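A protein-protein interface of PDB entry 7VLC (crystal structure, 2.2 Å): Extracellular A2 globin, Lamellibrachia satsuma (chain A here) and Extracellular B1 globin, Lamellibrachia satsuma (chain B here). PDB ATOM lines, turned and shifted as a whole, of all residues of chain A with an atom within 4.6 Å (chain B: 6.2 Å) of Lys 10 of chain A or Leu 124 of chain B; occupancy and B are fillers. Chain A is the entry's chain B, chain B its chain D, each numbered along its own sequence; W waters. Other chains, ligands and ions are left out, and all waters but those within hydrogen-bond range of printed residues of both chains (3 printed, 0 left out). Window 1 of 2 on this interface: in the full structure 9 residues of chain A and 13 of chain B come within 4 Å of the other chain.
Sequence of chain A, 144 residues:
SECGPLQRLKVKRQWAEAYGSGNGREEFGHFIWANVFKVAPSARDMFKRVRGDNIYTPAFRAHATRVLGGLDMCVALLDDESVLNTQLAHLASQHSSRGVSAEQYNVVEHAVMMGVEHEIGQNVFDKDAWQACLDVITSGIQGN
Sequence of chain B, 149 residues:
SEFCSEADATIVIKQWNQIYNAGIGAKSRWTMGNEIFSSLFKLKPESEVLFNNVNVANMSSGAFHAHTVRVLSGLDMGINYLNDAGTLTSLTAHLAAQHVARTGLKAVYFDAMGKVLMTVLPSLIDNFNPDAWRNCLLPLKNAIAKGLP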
ATOM      1  N   LEU A   6     -10.093 -27.974 -15.113  1.00  0.00           N
ATOM      2  CA  LEU A   6      -9.973 -26.519 -15.138  1.00  0.00           C
ATOM      3  C   LEU A   6      -9.589 -25.970 -13.769  1.00  0.00           C
ATOM      4  O   LEU A   6      -8.742 -25.073 -13.670  1.00  0.00           O
ATOM      5  CB  LEU A   6     -11.284 -25.894 -15.615  1.00  0.00           C
ATOM      6  CG  LEU A   6     -11.768 -26.279 -17.015  1.00  0.00           C
ATOM      7  CD1 LEU A   6     -13.165 -25.728 -17.262  1.00  0.00           C
ATOM      8  CD2 LEU A   6     -10.801 -25.783 -18.079  1.00  0.00           C
ATOM      9  N   GLN A   7     -10.207 -26.490 -12.703  1.00  0.00           N
ATOM     10  CA  GLN A   7      -9.896 -26.019 -11.358  1.00  0.00           C
ATOM     11  C   GLN A   7      -8.468 -26.363 -10.961  1.00  0.00           C
ATOM     12  O   GLN A   7      -7.831 -25.600 -10.227  1.00  0.00           O
ATOM     13  CB  GLN A   7     -10.879 -26.606 -10.343  1.00  0.00           C
ATOM     14  CG  GLN A   7     -12.288 -26.020 -10.414  1.00  0.00           C
ATOM     15  CD  GLN A   7     -13.076 -26.521 -11.610  1.00  0.00           C
ATOM     16  OE1 GLN A   7     -12.819 -27.607 -12.127  1.00  0.00           O
ATOM     17  NE2 GLN A   7     -14.041 -25.726 -12.058  1.00  0.00           N
ATOM     18  N   ARG A   8      -7.954 -27.502 -11.433  1.00  0.00           N
ATOM     19  CA  ARG A   8      -6.571 -27.860 -11.144  1.00  0.00           C
ATOM     20  C   ARG A   8      -5.600 -26.882 -11.794  1.00  0.00           C
ATOM     21  O   ARG A   8      -4.589 -26.508 -11.187  1.00  0.00           O
ATOM     22  CB  ARG A   8      -6.297 -29.291 -11.606  1.00  0.00           C
ATOM     23  CG  ARG A   8      -6.979 -30.337 -10.744  1.00  0.00           C
ATOM     24  CD  ARG A   8      -7.170 -31.658 -11.470  1.00  0.00           C
ATOM     25  NE  ARG A   8      -8.102 -32.514 -10.744  1.00  0.00           N
ATOM     26  CZ  ARG A   8      -7.737 -33.500  -9.932  1.00  0.00           C
ATOM     27  NH1 ARG A   8      -6.451 -33.776  -9.752  1.00  0.00           N
ATOM     28  NH2 ARG A   8      -8.661 -34.215  -9.309  1.00  0.00           N
ATOM     29  N   LEU A   9      -5.894 -26.447 -13.024  1.00  0.00           N
ATOM     30  CA  LEU A   9      -5.042 -25.461 -13.682  1.00  0.00           C
ATOM     31  C   LEU A   9      -5.062 -24.124 -12.944  1.00  0.00           C
ATOM     32  O   LEU A   9      -4.008 -23.511 -12.734  1.00  0.00           O
ATOM     33  CB  LEU A   9      -5.474 -25.280 -15.137  1.00  0.00           C
ATOM     34  CG  LEU A   9      -5.314 -26.485 -16.072  1.00  0.00           C
ATOM     35  CD1 LEU A   9      -5.835 -26.155 -17.461  1.00  0.00           C
ATOM     36  CD2 LEU A   9      -3.863 -26.932 -16.142  1.00  0.00           C
ATOM     37  N   LYS A  10      -6.251 -23.657 -12.544  1.00  0.00           N
ATOM     38  CA  LYS A  10      -6.352 -22.390 -11.821  1.00  0.00           C
ATOM     39  C   LYS A  10      -5.617 -22.449 -10.487  1.00  0.00           C
ATOM     40  O   LYS A  10      -4.882 -21.518 -10.136  1.00  0.00           O
ATOM     41  CB  LYS A  10      -7.822 -22.026 -11.602  1.00  0.00           C
ATOM     42  CG  LYS A  10      -8.036 -20.842 -10.676  1.00  0.00           C
ATOM     43  CD  LYS A  10      -8.203 -19.539 -11.446  1.00  0.00           C
ATOM     44  CE  LYS A  10      -9.667 -19.279 -11.772  1.00  0.00           C
ATOM     45  NZ  LYS A  10      -9.924 -17.876 -12.211  1.00  0.00           N
ATOM     46  N   VAL A  11      -5.804 -23.534  -9.731  1.00  0.00           N
ATOM     47  CA  VAL A  11      -5.118 -23.687  -8.450  1.00  0.00           C
ATOM     48  C   VAL A  11      -3.608 -23.714  -8.648  1.00  0.00           C
ATOM     49  O   VAL A  11      -2.854 -23.151  -7.845  1.00  0.00           O
ATOM     50  CB  VAL A  11      -5.621 -24.947  -7.717  1.00  0.00           C
ATOM     51  CG1 VAL A  11      -4.692 -25.308  -6.561  1.00  0.00           C
ATOM     52  CG2 VAL A  11      -7.032 -24.726  -7.200  1.00  0.00           C
ATOM     53  N   LYS A  12      -3.144 -24.368  -9.719  1.00  0.00           N
ATOM     54  CA  LYS A  12      -1.714 -24.404 -10.015  1.00  0.00           C
ATOM     55  C   LYS A  12      -1.142 -22.997 -10.153  1.00  0.00           C
ATOM     56  O   LYS A  12      -0.174 -22.635  -9.472  1.00  0.00           O
ATOM     57  CB  LYS A  12      -1.461 -25.210 -11.291  1.00  0.00           C
ATOM     58  CG  LYS A  12      -1.415 -26.724 -11.103  1.00  0.00           C
ATOM     59  CD  LYS A  12      -1.412 -27.434 -12.447  1.00  0.00           C
ATOM     60  CE  LYS A  12      -1.119 -28.912 -12.301  1.00  0.00           C
ATOM     61  NZ  LYS A  12       0.323 -29.159 -12.036  1.00  0.00           N
ATOM     62  N   ARG A  13      -1.737 -22.186 -11.029  1.00  0.00           N
ATOM     63  CA  ARG A  13      -1.208 -20.850 -11.280  1.00  0.00           C
ATOM     64  C   ARG A  13      -1.327 -19.965 -10.045  1.00  0.00           C
ATOM     65  O   ARG A  13      -0.405 -19.208  -9.727  1.00  0.00           O
ATOM     66  CB  ARG A  13      -1.929 -20.222 -12.474  1.00  0.00           C
ATOM     67  CG  ARG A  13      -1.423 -18.847 -12.859  1.00  0.00           C
ATOM     68  CD  ARG A  13      -2.186 -18.310 -14.055  1.00  0.00           C
ATOM     69  NE  ARG A  13      -3.630 -18.405 -13.858  1.00  0.00           N
ATOM     70  CZ  ARG A  13      -4.351 -17.528 -13.167  1.00  0.00           C
ATOM     71  NH1 ARG A  13      -5.660 -17.697 -13.042  1.00  0.00           N
ATOM     72  NH2 ARG A  13      -3.765 -16.483 -12.598  1.00  0.00           N
ATOM     73  N   GLN A  14      -2.446 -20.059  -9.320  1.00  0.00           N
ATOM     74  CA  GLN A  14      -2.600 -19.248  -8.117  1.00  0.00           C
ATOM     75  C   GLN A  14      -1.635 -19.674  -7.021  1.00  0.00           C
ATOM     76  O   GLN A  14      -1.155 -18.824  -6.261  1.00  0.00           O
ATOM     77  CB  GLN A  14      -4.043 -19.306  -7.615  1.00  0.00           C
ATOM     78  CG  GLN A  14      -5.015 -18.521  -8.476  1.00  0.00           C
ATOM     79  CD  GLN A  14      -6.342 -18.274  -7.789  1.00  0.00           C
ATOM     80  OE1 GLN A  14      -6.641 -18.874  -6.754  1.00  0.00           O
ATOM     81  NE2 GLN A  14      -7.145 -17.382  -8.356  1.00  0.00           N
ATOM     82  N   ASP A 126      -9.921 -17.918  -5.984  1.00  0.00           N
ATOM     83  CA  ASP A 126     -10.986 -18.823  -6.414  1.00  0.00           C
ATOM     84  C   ASP A 126     -11.235 -19.803  -5.275  1.00  0.00           C
ATOM     85  O   ASP A 126     -10.552 -20.822  -5.157  1.00  0.00           O
ATOM     86  CB  ASP A 126     -10.606 -19.538  -7.708  1.00  0.00           C
ATOM     87  CG  ASP A 126     -11.797 -20.202  -8.392  1.00  0.00           C
ATOM     88  OD1 ASP A 126     -12.669 -20.762  -7.693  1.00  0.00           O
ATOM     89  OD2 ASP A 126     -11.857 -20.164  -9.638  1.00  0.00           O
ATOM     90  N   GLN B  18      -2.202 -14.889 -19.506  1.00  0.00           N
ATOM     91  CA  GLN B  18      -2.222 -15.425 -18.152  1.00  0.00           C
ATOM     92  C   GLN B  18      -2.369 -16.944 -18.151  1.00  0.00           C
ATOM     93  O   GLN B  18      -1.764 -17.633 -17.323  1.00  0.00           O
ATOM     94  CB  GLN B  18      -3.367 -14.758 -17.393  1.00  0.00           C
ATOM     95  CG  GLN B  18      -3.554 -15.143 -15.954  1.00  0.00           C
ATOM     96  CD  GLN B  18      -4.752 -14.428 -15.355  1.00  0.00           C
ATOM     97  OE1 GLN B  18      -5.441 -14.964 -14.491  1.00  0.00           O
ATOM     98  NE2 GLN B  18      -5.009 -13.211 -15.824  1.00  0.00           N
ATOM     99  N   ILE B  19      -3.171 -17.484 -19.068  1.00  0.00           N
ATOM    100  CA  ILE B  19      -3.417 -18.923 -19.127  1.00  0.00           C
ATOM    101  C   ILE B  19      -2.811 -19.579 -20.357  1.00  0.00           C
ATOM    102  O   ILE B  19      -2.843 -20.817 -20.454  1.00  0.00           O
ATOM    103  CB  ILE B  19      -4.923 -19.245 -19.065  1.00  0.00           C
ATOM    104  CG1 ILE B  19      -5.641 -18.638 -20.272  1.00  0.00           C
ATOM    105  CG2 ILE B  19      -5.529 -18.732 -17.772  1.00  0.00           C
ATOM    106  CD1 ILE B  19      -7.050 -19.152 -20.472  1.00  0.00           C
ATOM    107  N   MET B  32      -7.122 -27.690 -21.857  1.00  0.00           N
ATOM    108  CA  MET B  32      -8.089 -26.649 -22.182  1.00  0.00           C
ATOM    109  C   MET B  32      -8.813 -26.961 -23.486  1.00  0.00           C
ATOM    110  O   MET B  32     -10.022 -26.729 -23.602  1.00  0.00           O
ATOM    111  CB  MET B  32      -7.393 -25.292 -22.272  1.00  0.00           C
ATOM    112  CG  MET B  32      -6.854 -24.766 -20.953  1.00  0.00           C
ATOM    113  SD  MET B  32      -5.833 -23.300 -21.194  1.00  0.00           S
ATOM    114  CE  MET B  32      -6.905 -22.312 -22.233  1.00  0.00           C
ATOM    115  N   VAL B 120     -15.969 -21.430 -20.207  1.00  0.00           N
ATOM    116  CA  VAL B 120     -14.769 -22.087 -19.697  1.00  0.00           C
ATOM    117  C   VAL B 120     -13.770 -21.069 -19.157  1.00  0.00           C
ATOM    118  O   VAL B 120     -13.196 -21.257 -18.078  1.00  0.00           O
ATOM    119  CB  VAL B 120     -14.137 -22.959 -20.800  1.00  0.00           C
ATOM    120  CG1 VAL B 120     -12.794 -23.508 -20.343  1.00  0.00           C
ATOM    121  CG2 VAL B 120     -15.079 -24.094 -21.204  1.00  0.00           C
ATOM    122  N   LEU B 121     -13.537 -19.987 -19.902  1.00  0.00           N
ATOM    123  CA  LEU B 121     -12.453 -19.066 -19.560  1.00  0.00           C
ATOM    124  C   LEU B 121     -12.559 -18.461 -18.162  1.00  0.00           C
ATOM    125  O   LEU B 121     -11.513 -18.339 -17.501  1.00  0.00           O
ATOM    126  CB  LEU B 121     -12.360 -17.961 -20.621  1.00  0.00           C
ATOM    127  CG  LEU B 121     -11.903 -18.429 -22.005  1.00  0.00           C
ATOM    128  CD1 LEU B 121     -11.900 -17.272 -22.985  1.00  0.00           C
ATOM    129  CD2 LEU B 121     -10.527 -19.083 -21.937  1.00  0.00           C
ATOM    130  N   PRO B 122     -13.734 -18.067 -17.653  1.00  0.00           N
ATOM    131  CA  PRO B 122     -13.776 -17.563 -16.268  1.00  0.00           C
ATOM    132  C   PRO B 122     -13.305 -18.575 -15.239  1.00  0.00           C
ATOM    133  O   PRO B 122     -12.811 -18.175 -14.178  1.00  0.00           O
ATOM    134  CB  PRO B 122     -15.254 -17.194 -16.066  1.00  0.00           C
ATOM    135  CG  PRO B 122     -15.985 -17.844 -17.185  1.00  0.00           C
ATOM    136  CD  PRO B 122     -15.029 -17.880 -18.325  1.00  0.00           C
ATOM    137  N   SER B 123     -13.433 -19.873 -15.522  1.00  0.00           N
ATOM    138  CA  SER B 123     -12.913 -20.890 -14.615  1.00  0.00           C
ATOM    139  C   SER B 123     -11.393 -20.960 -14.621  1.00  0.00           C
ATOM    140  O   SER B 123     -10.819 -21.592 -13.729  1.00  0.00           O
ATOM    141  CB  SER B 123     -13.480 -22.263 -14.979  1.00  0.00           C
ATOM    142  OG  SER B 123     -14.886 -22.205 -15.100  1.00  0.00           O
ATOM    143  N   LEU B 124     -10.738 -20.340 -15.602  1.00  0.00           N
ATOM    144  CA  LEU B 124      -9.287 -20.372 -15.736  1.00  0.00           C
ATOM    145  C   LEU B 124      -8.617 -19.034 -15.475  1.00  0.00           C
ATOM    146  O   LEU B 124      -7.464 -19.011 -15.041  1.00  0.00           O
ATOM    147  CB  LEU B 124      -8.894 -20.837 -17.145  1.00  0.00           C
ATOM    148  CG  LEU B 124      -9.212 -22.276 -17.542  1.00  0.00           C
ATOM    149  CD1 LEU B 124      -9.141 -22.416 -19.053  1.00  0.00           C
ATOM    150  CD2 LEU B 124      -8.252 -23.249 -16.864  1.00  0.00           C
ATOM    151  N   ILE B 125      -9.310 -17.928 -15.723  1.00  0.00           N
ATOM    152  CA  ILE B 125      -8.709 -16.599 -15.749  1.00  0.00           C
ATOM    153  C   ILE B 125      -9.090 -15.837 -14.485  1.00  0.00           C
ATOM    154  O   ILE B 125     -10.238 -15.901 -14.030  1.00  0.00           O
ATOM    155  CB  ILE B 125      -9.146 -15.843 -17.020  1.00  0.00           C
ATOM    156  CG1 ILE B 125      -8.584 -16.542 -18.261  1.00  0.00           C
ATOM    157  CG2 ILE B 125      -8.715 -14.381 -16.975  1.00  0.00           C
ATOM    158  CD1 ILE B 125      -8.911 -15.838 -19.569  1.00  0.00           C
ATOM    159  N   ASP B 126      -8.119 -15.122 -13.915  1.00  0.00           N
ATOM    160  CA  ASP B 126      -8.393 -14.237 -12.787  1.00  0.00           C
ATOM    161  C   ASP B 126      -9.101 -12.977 -13.268  1.00  0.00           C
ATOM    162  O   ASP B 126      -8.667 -12.344 -14.236  1.00  0.00           O
ATOM    163  CB  ASP B 126      -7.096 -13.856 -12.074  1.00  0.00           C
ATOM    164  CG  ASP B 126      -6.461 -15.017 -11.352  1.00  0.00           C
ATOM    165  OD1 ASP B 126      -7.102 -16.086 -11.252  1.00  0.00           O
ATOM    166  OD2 ASP B 126      -5.313 -14.855 -10.883  1.00  0.00           O
ATOM    167  N   ASN B 127     -10.180 -12.605 -12.579  1.00  0.00           N
ATOM    168  CA  ASN B 127     -10.949 -11.401 -12.900  1.00  0.00           C
ATOM    169  C   ASN B 127     -11.350 -11.370 -14.368  1.00  0.00           C
ATOM    170  O   ASN B 127     -11.144 -10.378 -15.071  1.00  0.00           O
ATOM    171  CB  ASN B 127     -10.176 -10.137 -12.535  1.00  0.00           C
ATOM    172  CG  ASN B 127     -10.369  -9.738 -11.102  1.00  0.00           C
ATOM    173  OD1 ASN B 127      -9.400  -9.522 -10.377  1.00  0.00           O
ATOM    174  ND2 ASN B 127     -11.623  -9.637 -10.678  1.00  0.00           N
HETATM  175  O   HOH W   1      -5.121 -20.616 -14.705  1.00  0.00           O
HETATM  176  O   HOH W   2     -11.659 -22.508 -11.269  1.00  0.00           O
HETATM  177  O   HOH W   3     -10.360 -15.587 -10.499  1.00  0.00           O
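NZ of Lys 10 of chain A lies within hydrogen-bond range of O of Ile 125 of chain B (2.7 Å).
The side-chain carboxylate of Asp 126 of chain B is in salt-bridge range of the side-chain amino group of Lys 10 of chain A, 3.5 Å away.
The guanidinium group (NH2) of Arg 13 of chain A lies within hydrogen-bond range of the side-chain amide oxygen (OE1) of Gln 18 of chain B (2.9 Å).
NH1 of Arg 13 of chain A lies within hydrogen-bond range of O of Leu 124 of chain B.
The side-chain carboxylate (OD1) of Asp 126 of chain B is in salt-bridge range of the guanidinium group (NH1) of Arg 13 of chain A (2.8 Å).
The side-chain carboxylate (OD1) of Asp 126 of chain B lies within hydrogen-bond range of the side-chain amide nitrogen (NE2) of Gln 14 of chain A, 3.2 Å away.
Among the printed residues, pairs that only touch across the chains: Leu 6 of chain A with Val 120 of chain B (3.8 Å), Leu 6 of chain A with Leu 124 of chain B (3.7 Å), Leu 9 of chain A with Met 32 of chain B (3.9 Å), Leu 9 of chain A with Leu 124 of chain B (3.8 Å), Lys 10 of chain A with Pro 122 of chain B (3.5 Å), Lys 10 of chain A with Ser 123 of chain B (3.2 Å) and Lys 10 of chain A with Leu 124 of chain B (3.7 Å).
Of the printed residues of chain B, Leu 9 of chain A touches Met 32 and Leu 124.
Of chain B, only Pro 122 (3.5 Å), Ser 123 (3.2 Å), Leu 124 (3.7 Å), Ile 125 (2.7 Å) and Asp 126 (3.5 Å) come within 4 Å of Lys 10 of chain A.
Of the printed residues of chain A, Gln 18 of chain B touches Arg 13.
Ile 19 of chain B touches none of the printed residues of chain A.
Of the printed residues of chain A, Val 120 of chain B touches Leu 6 (3.8 Å).
Printed residues of chain A within 4 Å of Ser 123 of chain B: Lys 10 (3.2 Å).
Printed residues of chain A within 4 Å of Leu 124 of chain B: Leu 6, Leu 9, Lys 10 and Arg 13.
Of the printed residues of chain A, Asp 126 of chain B touches Lys 10, Arg 13 and Gln 14.
Asn 127 of chain B touches none of the printed residues of chain A.
The nearest residue of chain B that does not touch Lys 10 of chain A is Asn 127 of chain B (5.3 Å).
The nearest printed residue of chain A that does not touch Leu 124 of chain B is Gln 7 of chain A (5.6 Å).
Hydrophobic or aromatic side chains of chain A within 4 Å of the printed part of chain B: Leu 6 and Leu 9.
Among the printed residues, 13 pairs touch across the chains.
OD2 of Asp 126 of chain A is in salt-bridge range of NZ of Lys 10 of chain A (3.9 Å).
The side-chain amide oxygen (OE1) of Gln 18 of chain B is in hydrogen-bond range of the backbone NH (N) of Asp 126 of chain B, 2.7 Å away.
Water W2 lies within hydrogen-bond range of the backbone carbonyl oxygen (O) of Ser 123 of chain B (2.8 Å) and the side-chain carboxylate (OD2) of Asp 126 of chain A (2.9 Å).
Water W1 lies within hydrogen-bond range of NE of Arg 13 of chain A (2.8 Å) and O of Leu 124 of chain B (2.9 Å).
Water W3 lies within hydrogen-bond range of the side-chain amino group of Lys 10 of chain A and the side-chain carboxylate of Asp 126 of chain B.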
